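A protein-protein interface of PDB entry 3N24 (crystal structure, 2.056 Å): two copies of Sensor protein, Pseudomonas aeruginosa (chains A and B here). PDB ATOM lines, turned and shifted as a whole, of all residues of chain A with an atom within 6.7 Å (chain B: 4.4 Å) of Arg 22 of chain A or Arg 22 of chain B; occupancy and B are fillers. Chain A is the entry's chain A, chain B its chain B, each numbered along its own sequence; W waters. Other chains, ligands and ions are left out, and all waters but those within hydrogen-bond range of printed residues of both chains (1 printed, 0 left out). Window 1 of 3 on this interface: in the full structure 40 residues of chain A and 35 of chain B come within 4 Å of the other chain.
Among the printed residues, pairs that only touch across the chains: Gln 109 of chain A with Arg 22 of chain B, Gln 112 of chain A with Ser 18 of chain B, Leu 108 of chain A with Ser 18 of chain B, Ser 18 of chain A with Gln 112 of chain B, Arg 22 of chain A with Leu 108 of chain B, Leu 108 of chain A with Arg 22 of chain B, Leu 108 of chain A with Leu 21 of chain B and Leu 21 of chain A with Leu 108 of chain B.
The side-chain amide oxygen (OE1) of Gln 112 of chain A sits at hydrogen-bond distance from the guanidinium group (NH1) of Arg 22 of chain B (2.9 Å). The side-chain amide oxygen (OE1) of Gln 19 of chain B lies within hydrogen-bond range of the side-chain amide nitrogen (NE2) of Gln 112 of chain A (3.1 Å). The side-chain amide nitrogen (NE2) of Gln 19 of chain A lies within hydrogen-bond range of the side-chain amide oxygen (OE1) of Gln 112 of chain B. The guanidinium group (NH1) of Arg 22 of chain A is in hydrogen-bond range of the side-chain amide oxygen (OE1) of Gln 19 of chain B, at 3.0 Å. The side-chain amide oxygen (OE1) of Gln 112 of chain B sits at hydrogen-bond distance from the guanidinium group (NH1) of Arg 22 of chain A, 3.4 Å away. The side-chain amide nitrogen (NE2) of Gln 112 of chain B lies within hydrogen-bond range of the side-chain amide oxygen (OE1) of Gln 112 of chain A (3.0 Å). The side-chain amide oxygen (OE1) of Gln 19 of chain A sits at hydrogen-bond distance from the guanidinium group (NH1) of Arg 22 of chain B, at 3.1 Å. NH1 of Arg 22 of chain B lies close to NH1 of Arg 22 of chain A, 3.4 Å away.
Printed residues of chain B that touch a printed residue of chain A: Ser 18, Gln 19, Leu 21, Arg 22, Leu 108 and Gln 112. Hydrophobic or aromatic side chains of chain B that line the printed part of chain A: Leu 21 and Leu 108. Of the 18 printed residues of chain A, 7 touch a printed residue of chain B. Printed residues of chain A that touch a printed residue of chain B: Ser 18, Gln 19, Leu 21, Arg 22, Leu 108, Gln 109 and Gln 112. Hydrophobic or aromatic side chains of chain A within 4 Å of the printed part of chain B: Leu 21 and Leu 108. Among the printed residues, 16 pairs touch across the chains. Among the printed residues, no Asp or Glu carboxylate lies within 4 Å of a Lys or Arg side-chain nitrogen of the other chain.
Of chain B, only Gln 19 (3.0 Å), Arg 22 (3.4 Å), Leu 108 (3.8 Å) and Gln 112 (3.4 Å) come within 4 Å of Arg 22 of chain A. Printed residues of chain B within 4 Å of Gln 109 of chain A: Arg 22. Printed residues of chain A within 4 Å of Ser 18 of chain B: Leu 108 (3.6 Å) and Gln 112 (3.5 Å). Of chain A, only Gln 19, Arg 22, Leu 108, Gln 109 and Gln 112 come within 4 Å of Arg 22 of chain B. Printed residues of chain A within 4 Å of Gln 112 of chain B: Ser 18 (3.6 Å), Gln 19 (2.9 Å), Arg 22 (3.4 Å) and Gln 112 (3.0 Å). The nearest printed residue of chain B that does not touch Arg 22 of chain A is Gln 23 of chain B (5.2 Å). The nearest residue of chain A that does not touch Arg 22 of chain B is Gln 23 of chain A (4.9 Å).
NE2 of Gln 19 of chain B lies close to NE2 of Gln 112 of chain B, at 2.9 Å. The side-chain amide nitrogen of Gln 19 of chain A sits at hydrogen-bond distance from the side-chain amide oxygen of Gln 112 of chain A, at 2.6 Å. OE1 of Gln 113 of chain A lies close to OE1 of Gln 19 of chain A.
Water W1 lies within hydrogen-bond range of the side-chain amide oxygen (OE1) of Gln 19 of chain B (2.6 Å) and the guanidinium group (NH2) of Arg 22 of chain A (2.9 Å).
Ser 18 of chain A touches Gln 112 of chain B, and with the chains exchanged Gln 112 of chain A touches Ser 18 of chain B. Leu 21 of chain A touches Leu 108 of chain B, and with the chains exchanged Leu 108 of chain A touches Leu 21 of chain B. Arg 22 of chain A touches Leu 108 of chain B, and with the chains exchanged Leu 108 of chain A touches Arg 22 of chain B. Arg 22 of chain A touches Gln 112 of chain B, and with the chains exchanged Gln 112 of chain A touches Arg 22 of chain B. Of the 16 pairs that touch across the chains among the printed residues, 14 have their exchanged pair printed and touching as well.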
ATOM      1  N   VAL A  17      -4.733  34.528 -27.258  1.00  0.00           N
ATOM      2  CA  VAL A  17      -3.357  34.083 -26.999  1.00  0.00           C
ATOM      3  C   VAL A  17      -3.334  32.688 -26.332  1.00  0.00           C
ATOM      4  O   VAL A  17      -2.601  31.788 -26.756  1.00  0.00           O
ATOM      5  CB  VAL A  17      -2.602  35.070 -26.081  1.00  0.00           C
ATOM      6  CG1 VAL A  17      -1.358  34.415 -25.494  1.00  0.00           C
ATOM      7  CG2 VAL A  17      -2.259  36.350 -26.813  1.00  0.00           C
ATOM      8  N   SER A  18      -4.142  32.519 -25.284  1.00  0.00           N
ATOM      9  CA  SER A  18      -4.163  31.268 -24.539  1.00  0.00           C
ATOM     10  C   SER A  18      -4.620  30.111 -25.435  1.00  0.00           C
ATOM     11  O   SER A  18      -4.132  28.998 -25.310  1.00  0.00           O
ATOM     12  CB  SER A  18      -5.048  31.376 -23.295  1.00  0.00           C
ATOM     13  OG  SER A  18      -6.413  31.501 -23.654  1.00  0.00           O
ATOM     14  N   GLN A  19      -5.554  30.391 -26.337  1.00  0.00           N
ATOM     15  CA  GLN A  19      -6.030  29.387 -27.289  1.00  0.00           C
ATOM     16  C   GLN A  19      -4.938  28.964 -28.269  1.00  0.00           C
ATOM     17  O   GLN A  19      -4.713  27.778 -28.473  1.00  0.00           O
ATOM     18  CB  GLN A  19      -7.255  29.905 -28.047  1.00  0.00           C
ATOM     19  CG  GLN A  19      -8.529  29.954 -27.208  1.00  0.00           C
ATOM     20  CD  GLN A  19      -9.107  28.568 -26.953  1.00  0.00           C
ATOM     21  OE1 GLN A  19      -8.643  27.578 -27.508  1.00  0.00           O
ATOM     22  NE2 GLN A  19     -10.129  28.498 -26.114  1.00  0.00           N
ATOM     23  N   GLN A  20      -4.249  29.931 -28.867  1.00  0.00           N
ATOM     24  CA  GLN A  20      -3.114  29.612 -29.750  1.00  0.00           C
ATOM     25  C   GLN A  20      -1.995  28.857 -29.029  1.00  0.00           C
ATOM     26  O   GLN A  20      -1.385  27.942 -29.576  1.00  0.00           O
ATOM     27  CB  GLN A  20      -2.544  30.888 -30.379  1.00  0.00           C
ATOM     28  CG  GLN A  20      -3.256  31.336 -31.655  1.00  0.00           C
ATOM     29  CD  GLN A  20      -2.718  32.655 -32.218  1.00  0.00           C
ATOM     30  OE1 GLN A  20      -1.704  33.189 -31.750  1.00  0.00           O
ATOM     31  NE2 GLN A  20      -3.405  33.183 -33.231  1.00  0.00           N
ATOM     32  N   LEU A  21      -1.700  29.255 -27.798  1.00  0.00           N
ATOM     33  CA  LEU A  21      -0.670  28.575 -27.046  1.00  0.00           C
ATOM     34  C   LEU A  21      -1.049  27.124 -26.714  1.00  0.00           C
ATOM     35  O   LEU A  21      -0.203  26.226 -26.755  1.00  0.00           O
ATOM     36  CB  LEU A  21      -0.337  29.365 -25.782  1.00  0.00           C
ATOM     37  CG  LEU A  21       0.426  30.669 -26.027  1.00  0.00           C
ATOM     38  CD1 LEU A  21       0.740  31.352 -24.744  1.00  0.00           C
ATOM     39  CD2 LEU A  21       1.733  30.456 -26.808  1.00  0.00           C
ATOM     40  N   ARG A  22      -2.317  26.898 -26.390  1.00  0.00           N
ATOM     41  CA  ARG A  22      -2.798  25.545 -26.102  1.00  0.00           C
ATOM     42  C   ARG A  22      -2.812  24.723 -27.359  1.00  0.00           C
ATOM     43  O   ARG A  22      -2.506  23.541 -27.337  1.00  0.00           O
ATOM     44  CB  ARG A  22      -4.202  25.580 -25.498  1.00  0.00           C
ATOM     45  CG  ARG A  22      -4.227  26.213 -24.125  1.00  0.00           C
ATOM     46  CD  ARG A  22      -5.649  26.505 -23.669  1.00  0.00           C
ATOM     47  NE  ARG A  22      -6.238  25.331 -23.035  1.00  0.00           N
ATOM     48  CZ  ARG A  22      -7.477  25.272 -22.551  1.00  0.00           C
ATOM     49  NH1 ARG A  22      -8.294  26.317 -22.656  1.00  0.00           N
ATOM     50  NH2 ARG A  22      -7.903  24.153 -21.972  1.00  0.00           N
ATOM     51  N   GLN A  23      -3.183  25.345 -28.469  1.00  0.00           N
ATOM     52  CA  GLN A  23      -3.131  24.661 -29.760  1.00  0.00           C
ATOM     53  C   GLN A  23      -1.703  24.239 -30.105  1.00  0.00           C
ATOM     54  O   GLN A  23      -1.456  23.113 -30.542  1.00  0.00           O
ATOM     55  CB  GLN A  23      -3.706  25.562 -30.849  1.00  0.00           C
ATOM     56  CG  GLN A  23      -3.806  24.904 -32.220  1.00  0.00           C
ATOM     57  CD  GLN A  23      -4.312  25.874 -33.263  1.00  0.00           C
ATOM     58  OE1 GLN A  23      -3.648  26.122 -34.268  1.00  0.00           O
ATOM     59  NE2 GLN A  23      -5.481  26.455 -33.013  1.00  0.00           N
ATOM     60  N   LEU A  24      -0.757  25.141 -29.884  1.00  0.00           N
ATOM     61  CA  LEU A  24       0.657  24.868 -30.167  1.00  0.00           C
ATOM     62  C   LEU A  24       1.223  23.832 -29.212  1.00  0.00           C
ATOM     63  O   LEU A  24       2.040  23.007 -29.604  1.00  0.00           O
ATOM     64  CB  LEU A  24       1.460  26.153 -30.060  1.00  0.00           C
ATOM     65  CG  LEU A  24       1.181  27.120 -31.200  1.00  0.00           C
ATOM     66  CD1 LEU A  24       1.772  28.508 -30.905  1.00  0.00           C
ATOM     67  CD2 LEU A  24       1.746  26.524 -32.487  1.00  0.00           C
ATOM     68  N   LEU A  25       0.789  23.878 -27.954  1.00  0.00           N
ATOM     69  CA  LEU A  25       1.196  22.854 -26.990  1.00  0.00           C
ATOM     70  C   LEU A  25       0.641  21.507 -27.445  1.00  0.00           C
ATOM     71  O   LEU A  25       1.341  20.494 -27.445  1.00  0.00           O
ATOM     72  CB  LEU A  25       0.670  23.178 -25.589  1.00  0.00           C
ATOM     73  CG  LEU A  25       0.996  22.111 -24.538  1.00  0.00           C
ATOM     74  CD1 LEU A  25       2.508  21.806 -24.547  1.00  0.00           C
ATOM     75  CD2 LEU A  25       0.527  22.581 -23.193  1.00  0.00           C
ATOM     76  N   GLY A  26      -0.626  21.514 -27.849  1.00  0.00           N
ATOM     77  CA  GLY A  26      -1.221  20.353 -28.481  1.00  0.00           C
ATOM     78  C   GLY A  26      -0.418  19.812 -29.661  1.00  0.00           C
ATOM     79  O   GLY A  26      -0.176  18.608 -29.731  1.00  0.00           O
ATOM     80  N   ASP A  27      -0.032  20.691 -30.588  1.00  0.00           N
ATOM     81  CA  ASP A  27       0.794  20.304 -31.740  1.00  0.00           C
ATOM     82  C   ASP A  27       2.027  19.510 -31.287  1.00  0.00           C
ATOM     83  O   ASP A  27       2.343  18.467 -31.851  1.00  0.00           O
ATOM     84  CB  ASP A  27       1.275  21.545 -32.519  1.00  0.00           C
ATOM     85  CG  ASP A  27       0.148  22.289 -33.215  1.00  0.00           C
ATOM     86  OD1 ASP A  27      -0.913  21.690 -33.416  1.00  0.00           O
ATOM     87  OD2 ASP A  27       0.324  23.480 -33.565  1.00  0.00           O
ATOM     88  N   PHE A  49       5.809  28.333 -30.424  1.00  0.00           N
ATOM     89  CA  PHE A  49       5.229  28.592 -29.119  1.00  0.00           C
ATOM     90  C   PHE A  49       5.881  29.836 -28.527  1.00  0.00           C
ATOM     91  O   PHE A  49       5.193  30.756 -28.110  1.00  0.00           O
ATOM     92  CB  PHE A  49       5.373  27.395 -28.183  1.00  0.00           C
ATOM     93  CG  PHE A  49       4.606  27.543 -26.889  1.00  0.00           C
ATOM     94  CD1 PHE A  49       3.450  26.826 -26.667  1.00  0.00           C
ATOM     95  CD2 PHE A  49       5.052  28.404 -25.901  1.00  0.00           C
ATOM     96  CE1 PHE A  49       2.753  26.947 -25.467  1.00  0.00           C
ATOM     97  CE2 PHE A  49       4.350  28.544 -24.709  1.00  0.00           C
ATOM     98  CZ  PHE A  49       3.208  27.817 -24.492  1.00  0.00           C
ATOM     99  N   ARG A 105      -8.761  16.862 -29.752  1.00  0.00           N
ATOM    100  CA  ARG A 105      -8.491  18.200 -29.210  1.00  0.00           C
ATOM    101  C   ARG A 105      -8.980  19.309 -30.141  1.00  0.00           C
ATOM    102  O   ARG A 105      -9.413  20.366 -29.687  1.00  0.00           O
ATOM    103  CB  ARG A 105      -7.021  18.383 -28.822  1.00  0.00           C
ATOM    104  CG  ARG A 105      -6.024  18.112 -29.923  1.00  0.00           C
ATOM    105  CD  ARG A 105      -5.425  19.381 -30.482  1.00  0.00           C
ATOM    106  NE  ARG A 105      -4.397  19.095 -31.488  1.00  0.00           N
ATOM    107  CZ  ARG A 105      -3.426  19.943 -31.822  1.00  0.00           C
ATOM    108  NH1 ARG A 105      -2.536  19.620 -32.755  1.00  0.00           N
ATOM    109  NH2 ARG A 105      -3.346  21.120 -31.217  1.00  0.00           N
ATOM    110  N   LEU A 108     -12.625  19.956 -29.588  1.00  0.00           N
ATOM    111  CA  LEU A 108     -12.922  20.592 -28.315  1.00  0.00           C
ATOM    112  C   LEU A 108     -12.573  22.079 -28.413  1.00  0.00           C
ATOM    113  O   LEU A 108     -13.317  22.919 -27.925  1.00  0.00           O
ATOM    114  CB  LEU A 108     -12.174  19.889 -27.160  1.00  0.00           C
ATOM    115  CG  LEU A 108     -12.700  18.494 -26.800  1.00  0.00           C
ATOM    116  CD1 LEU A 108     -11.791  17.783 -25.813  1.00  0.00           C
ATOM    117  CD2 LEU A 108     -14.137  18.582 -26.251  1.00  0.00           C
ATOM    118  N   GLN A 109     -11.450  22.380 -29.062  1.00  0.00           N
ATOM    119  CA  GLN A 109     -10.949  23.753 -29.240  1.00  0.00           C
ATOM    120  C   GLN A 109     -11.857  24.608 -30.119  1.00  0.00           C
ATOM    121  O   GLN A 109     -12.163  25.761 -29.792  1.00  0.00           O
ATOM    122  CB  GLN A 109      -9.577  23.725 -29.919  1.00  0.00           C
ATOM    123  CG  GLN A 109      -8.440  23.217 -29.085  1.00  0.00           C
ATOM    124  CD  GLN A 109      -7.096  23.401 -29.762  1.00  0.00           C
ATOM    125  OE1 GLN A 109      -6.083  22.876 -29.298  1.00  0.00           O
ATOM    126  NE2 GLN A 109      -7.080  24.149 -30.868  1.00  0.00           N
ATOM    127  N   ASP A 110     -12.240  24.043 -31.261  1.00  0.00           N
ATOM    128  CA  ASP A 110     -13.087  24.735 -32.223  1.00  0.00           C
ATOM    129  C   ASP A 110     -14.445  24.981 -31.592  1.00  0.00           C
ATOM    130  O   ASP A 110     -15.024  26.061 -31.733  1.00  0.00           O
ATOM    131  CB  ASP A 110     -13.232  23.908 -33.507  1.00  0.00           C
ATOM    132  CG  ASP A 110     -11.927  23.753 -34.247  1.00  0.00           C
ATOM    133  OD1 ASP A 110     -10.978  24.498 -33.930  1.00  0.00           O
ATOM    134  OD2 ASP A 110     -11.842  22.880 -35.134  1.00  0.00           O
ATOM    135  N   GLN A 112     -15.085  25.265 -28.364  1.00  0.00           N
ATOM    136  CA  GLN A 112     -14.972  26.345 -27.385  1.00  0.00           C
ATOM    137  C   GLN A 112     -14.782  27.732 -28.027  1.00  0.00           C
ATOM    138  O   GLN A 112     -15.392  28.703 -27.594  1.00  0.00           O
ATOM    139  CB  GLN A 112     -13.852  26.029 -26.397  1.00  0.00           C
ATOM    140  CG  GLN A 112     -13.769  26.929 -25.208  1.00  0.00           C
ATOM    141  CD  GLN A 112     -12.617  26.531 -24.307  1.00  0.00           C
ATOM    142  OE1 GLN A 112     -11.455  26.796 -24.616  1.00  0.00           O
ATOM    143  NE2 GLN A 112     -12.931  25.875 -23.191  1.00  0.00           N
ATOM    144  N   GLN A 113     -13.942  27.824 -29.054  1.00  0.00           N
ATOM    145  CA  GLN A 113     -13.664  29.108 -29.712  1.00  0.00           C
ATOM    146  C   GLN A 113     -14.852  29.657 -30.489  1.00  0.00           C
ATOM    147  O   GLN A 113     -14.857  30.815 -30.887  1.00  0.00           O
ATOM    148  CB  GLN A 113     -12.433  29.021 -30.634  1.00  0.00           C
ATOM    149  CG  GLN A 113     -11.126  29.319 -29.913  1.00  0.00           C
ATOM    150  CD  GLN A 113      -9.897  28.891 -30.694  1.00  0.00           C
ATOM    151  OE1 GLN A 113      -9.110  28.069 -30.229  1.00  0.00           O
ATOM    152  NE2 GLN A 113      -9.716  29.465 -31.871  1.00  0.00           N
ATOM    153  N   SER B  18     -16.929  22.710 -22.137  1.00  0.00           N
ATOM    154  CA  SER B  18     -15.781  22.599 -23.014  1.00  0.00           C
ATOM    155  C   SER B  18     -14.502  22.601 -22.198  1.00  0.00           C
ATOM    156  O   SER B  18     -13.583  21.821 -22.463  1.00  0.00           O
ATOM    157  CB  SER B  18     -15.757  23.767 -23.993  1.00  0.00           C
ATOM    158  OG  SER B  18     -15.734  23.295 -25.322  1.00  0.00           O
ATOM    159  N   GLN B  19     -14.436  23.489 -21.209  1.00  0.00           N
ATOM    160  CA  GLN B  19     -13.222  23.598 -20.421  1.00  0.00           C
ATOM    161  C   GLN B  19     -13.039  22.363 -19.542  1.00  0.00           C
ATOM    162  O   GLN B  19     -11.917  21.880 -19.368  1.00  0.00           O
ATOM    163  CB  GLN B  19     -13.213  24.876 -19.584  1.00  0.00           C
ATOM    164  CG  GLN B  19     -11.799  25.314 -19.143  1.00  0.00           C
ATOM    165  CD  GLN B  19     -10.934  25.854 -20.294  1.00  0.00           C
ATOM    166  OE1 GLN B  19     -10.659  25.154 -21.270  1.00  0.00           O
ATOM    167  NE2 GLN B  19     -10.504  27.105 -20.171  1.00  0.00           N
ATOM    168  N   GLN B  20     -14.144  21.852 -19.003  1.00  0.00           N
ATOM    169  CA  GLN B  20     -14.121  20.637 -18.191  1.00  0.00           C
ATOM    170  C   GLN B  20     -13.555  19.453 -18.977  1.00  0.00           C
ATOM    171  O   GLN B  20     -12.627  18.770 -18.517  1.00  0.00           O
ATOM    172  CB  GLN B  20     -15.525  20.296 -17.673  1.00  0.00           C
ATOM    173  CG  GLN B  20     -16.065  21.241 -16.608  1.00  0.00           C
ATOM    174  CD  GLN B  20     -17.267  20.651 -15.861  1.00  0.00           C
ATOM    175  OE1 GLN B  20     -18.423  20.881 -16.229  1.00  0.00           O
ATOM    176  NE2 GLN B  20     -16.989  19.880 -14.813  1.00  0.00           N
ATOM    177  N   LEU B  21     -14.095  19.220 -20.170  1.00  0.00           N
ATOM    178  CA  LEU B  21     -13.602  18.126 -20.996  1.00  0.00           C
ATOM    179  C   LEU B  21     -12.131  18.301 -21.346  1.00  0.00           C
ATOM    180  O   LEU B  21     -11.373  17.333 -21.337  1.00  0.00           O
ATOM    181  CB  LEU B  21     -14.428  17.965 -22.273  1.00  0.00           C
ATOM    182  CG  LEU B  21     -15.917  17.633 -22.086  1.00  0.00           C
ATOM    183  CD1 LEU B  21     -16.636  17.684 -23.411  1.00  0.00           C
ATOM    184  CD2 LEU B  21     -16.086  16.277 -21.431  1.00  0.00           C
ATOM    185  N   ARG B  22     -11.729  19.526 -21.658  1.00  0.00           N
ATOM    186  CA  ARG B  22     -10.341  19.772 -22.045  1.00  0.00           C
ATOM    187  C   ARG B  22      -9.451  19.483 -20.857  1.00  0.00           C
ATOM    188  O   ARG B  22      -8.395  18.873 -20.997  1.00  0.00           O
ATOM    189  CB  ARG B  22     -10.127  21.197 -22.562  1.00  0.00           C
ATOM    190  CG  ARG B  22     -10.626  21.411 -23.995  1.00  0.00           C
ATOM    191  CD  ARG B  22     -10.359  22.830 -24.511  1.00  0.00           C
ATOM    192  NE  ARG B  22      -9.028  22.977 -25.104  1.00  0.00           N
ATOM    193  CZ  ARG B  22      -8.588  24.100 -25.670  1.00  0.00           C
ATOM    194  NH1 ARG B  22      -9.361  25.172 -25.721  1.00  0.00           N
ATOM    195  NH2 ARG B  22      -7.366  24.158 -26.174  1.00  0.00           N
ATOM    196  N   GLN B  23      -9.895  19.898 -19.677  1.00  0.00           N
ATOM    197  CA  GLN B  23      -9.136  19.606 -18.473  1.00  0.00           C
ATOM    198  C   GLN B  23      -9.055  18.112 -18.220  1.00  0.00           C
ATOM    199  O   GLN B  23      -7.981  17.602 -17.931  1.00  0.00           O
ATOM    200  CB  GLN B  23      -9.709  20.329 -17.252  1.00  0.00           C
ATOM    201  CG  GLN B  23      -9.201  19.754 -15.933  1.00  0.00           C
ATOM    202  CD  GLN B  23      -8.757  20.823 -14.961  1.00  0.00           C
ATOM    203  OE1 GLN B  23      -7.965  20.566 -14.050  1.00  0.00           O
ATOM    204  NE2 GLN B  23      -9.264  22.034 -15.151  1.00  0.00           N
ATOM    205  N   LEU B  24     -10.183  17.403 -18.343  1.00  0.00           N
ATOM    206  CA  LEU B  24     -10.192  15.939 -18.158  1.00  0.00           C
ATOM    207  C   LEU B  24      -9.342  15.205 -19.181  1.00  0.00           C
ATOM    208  O   LEU B  24      -8.709  14.210 -18.864  1.00  0.00           O
ATOM    209  CB  LEU B  24     -11.615  15.375 -18.166  1.00  0.00           C
ATOM    210  CG  LEU B  24     -12.408  15.692 -16.907  1.00  0.00           C
ATOM    211  CD1 LEU B  24     -13.883  15.714 -17.194  1.00  0.00           C
ATOM    212  CD2 LEU B  24     -12.055  14.728 -15.781  1.00  0.00           C
ATOM    213  N   LEU B  25      -9.330  15.696 -20.417  1.00  0.00           N
ATOM    214  CA  LEU B  25      -8.432  15.163 -21.424  1.00  0.00           C
ATOM    215  C   LEU B  25      -6.981  15.382 -21.003  1.00  0.00           C
ATOM    216  O   LEU B  25      -6.154  14.479 -21.094  1.00  0.00           O
ATOM    217  CB  LEU B  25      -8.673  15.842 -22.776  1.00  0.00           C
ATOM    218  CG  LEU B  25      -7.709  15.423 -23.898  1.00  0.00           C
ATOM    219  CD1 LEU B  25      -7.480  13.916 -23.913  1.00  0.00           C
ATOM    220  CD2 LEU B  25      -8.244  15.903 -25.248  1.00  0.00           C
ATOM    221  N   GLY B  26      -6.671  16.594 -20.549  1.00  0.00           N
ATOM    222  CA  GLY B  26      -5.348  16.875 -20.036  1.00  0.00           C
ATOM    223  C   GLY B  26      -5.030  16.000 -18.834  1.00  0.00           C
ATOM    224  O   GLY B  26      -3.896  15.548 -18.675  1.00  0.00           O
ATOM    225  N   LEU B 108      -2.153  27.828 -18.537  1.00  0.00           N
ATOM    226  CA  LEU B 108      -2.879  28.246 -19.743  1.00  0.00           C
ATOM    227  C   LEU B 108      -4.375  28.162 -19.542  1.00  0.00           C
ATOM    228  O   LEU B 108      -5.130  29.034 -19.945  1.00  0.00           O
ATOM    229  CB  LEU B 108      -2.445  27.404 -20.946  1.00  0.00           C
ATOM    230  CG  LEU B 108      -0.991  27.683 -21.309  1.00  0.00           C
ATOM    231  CD1 LEU B 108      -0.461  26.645 -22.263  1.00  0.00           C
ATOM    232  CD2 LEU B 108      -0.842  29.097 -21.903  1.00  0.00           C
ATOM    233  N   GLN B 112      -6.943  31.547 -19.442  1.00  0.00           N
ATOM    234  CA  GLN B 112      -8.207  31.724 -20.144  1.00  0.00           C
ATOM    235  C   GLN B 112      -9.339  32.043 -19.186  1.00  0.00           C
ATOM    236  O   GLN B 112     -10.102  32.977 -19.420  1.00  0.00           O
ATOM    237  CB  GLN B 112      -8.561  30.501 -20.979  1.00  0.00           C
ATOM    238  CG  GLN B 112     -10.024  30.478 -21.383  1.00  0.00           C
ATOM    239  CD  GLN B 112     -10.294  29.486 -22.482  1.00  0.00           C
ATOM    240  OE1 GLN B 112      -9.523  29.377 -23.436  1.00  0.00           O
ATOM    241  NE2 GLN B 112     -11.387  28.741 -22.349  1.00  0.00           N
HETATM  242  O   HOH W   1      -9.421  23.580 -19.576  1.00  0.00           O
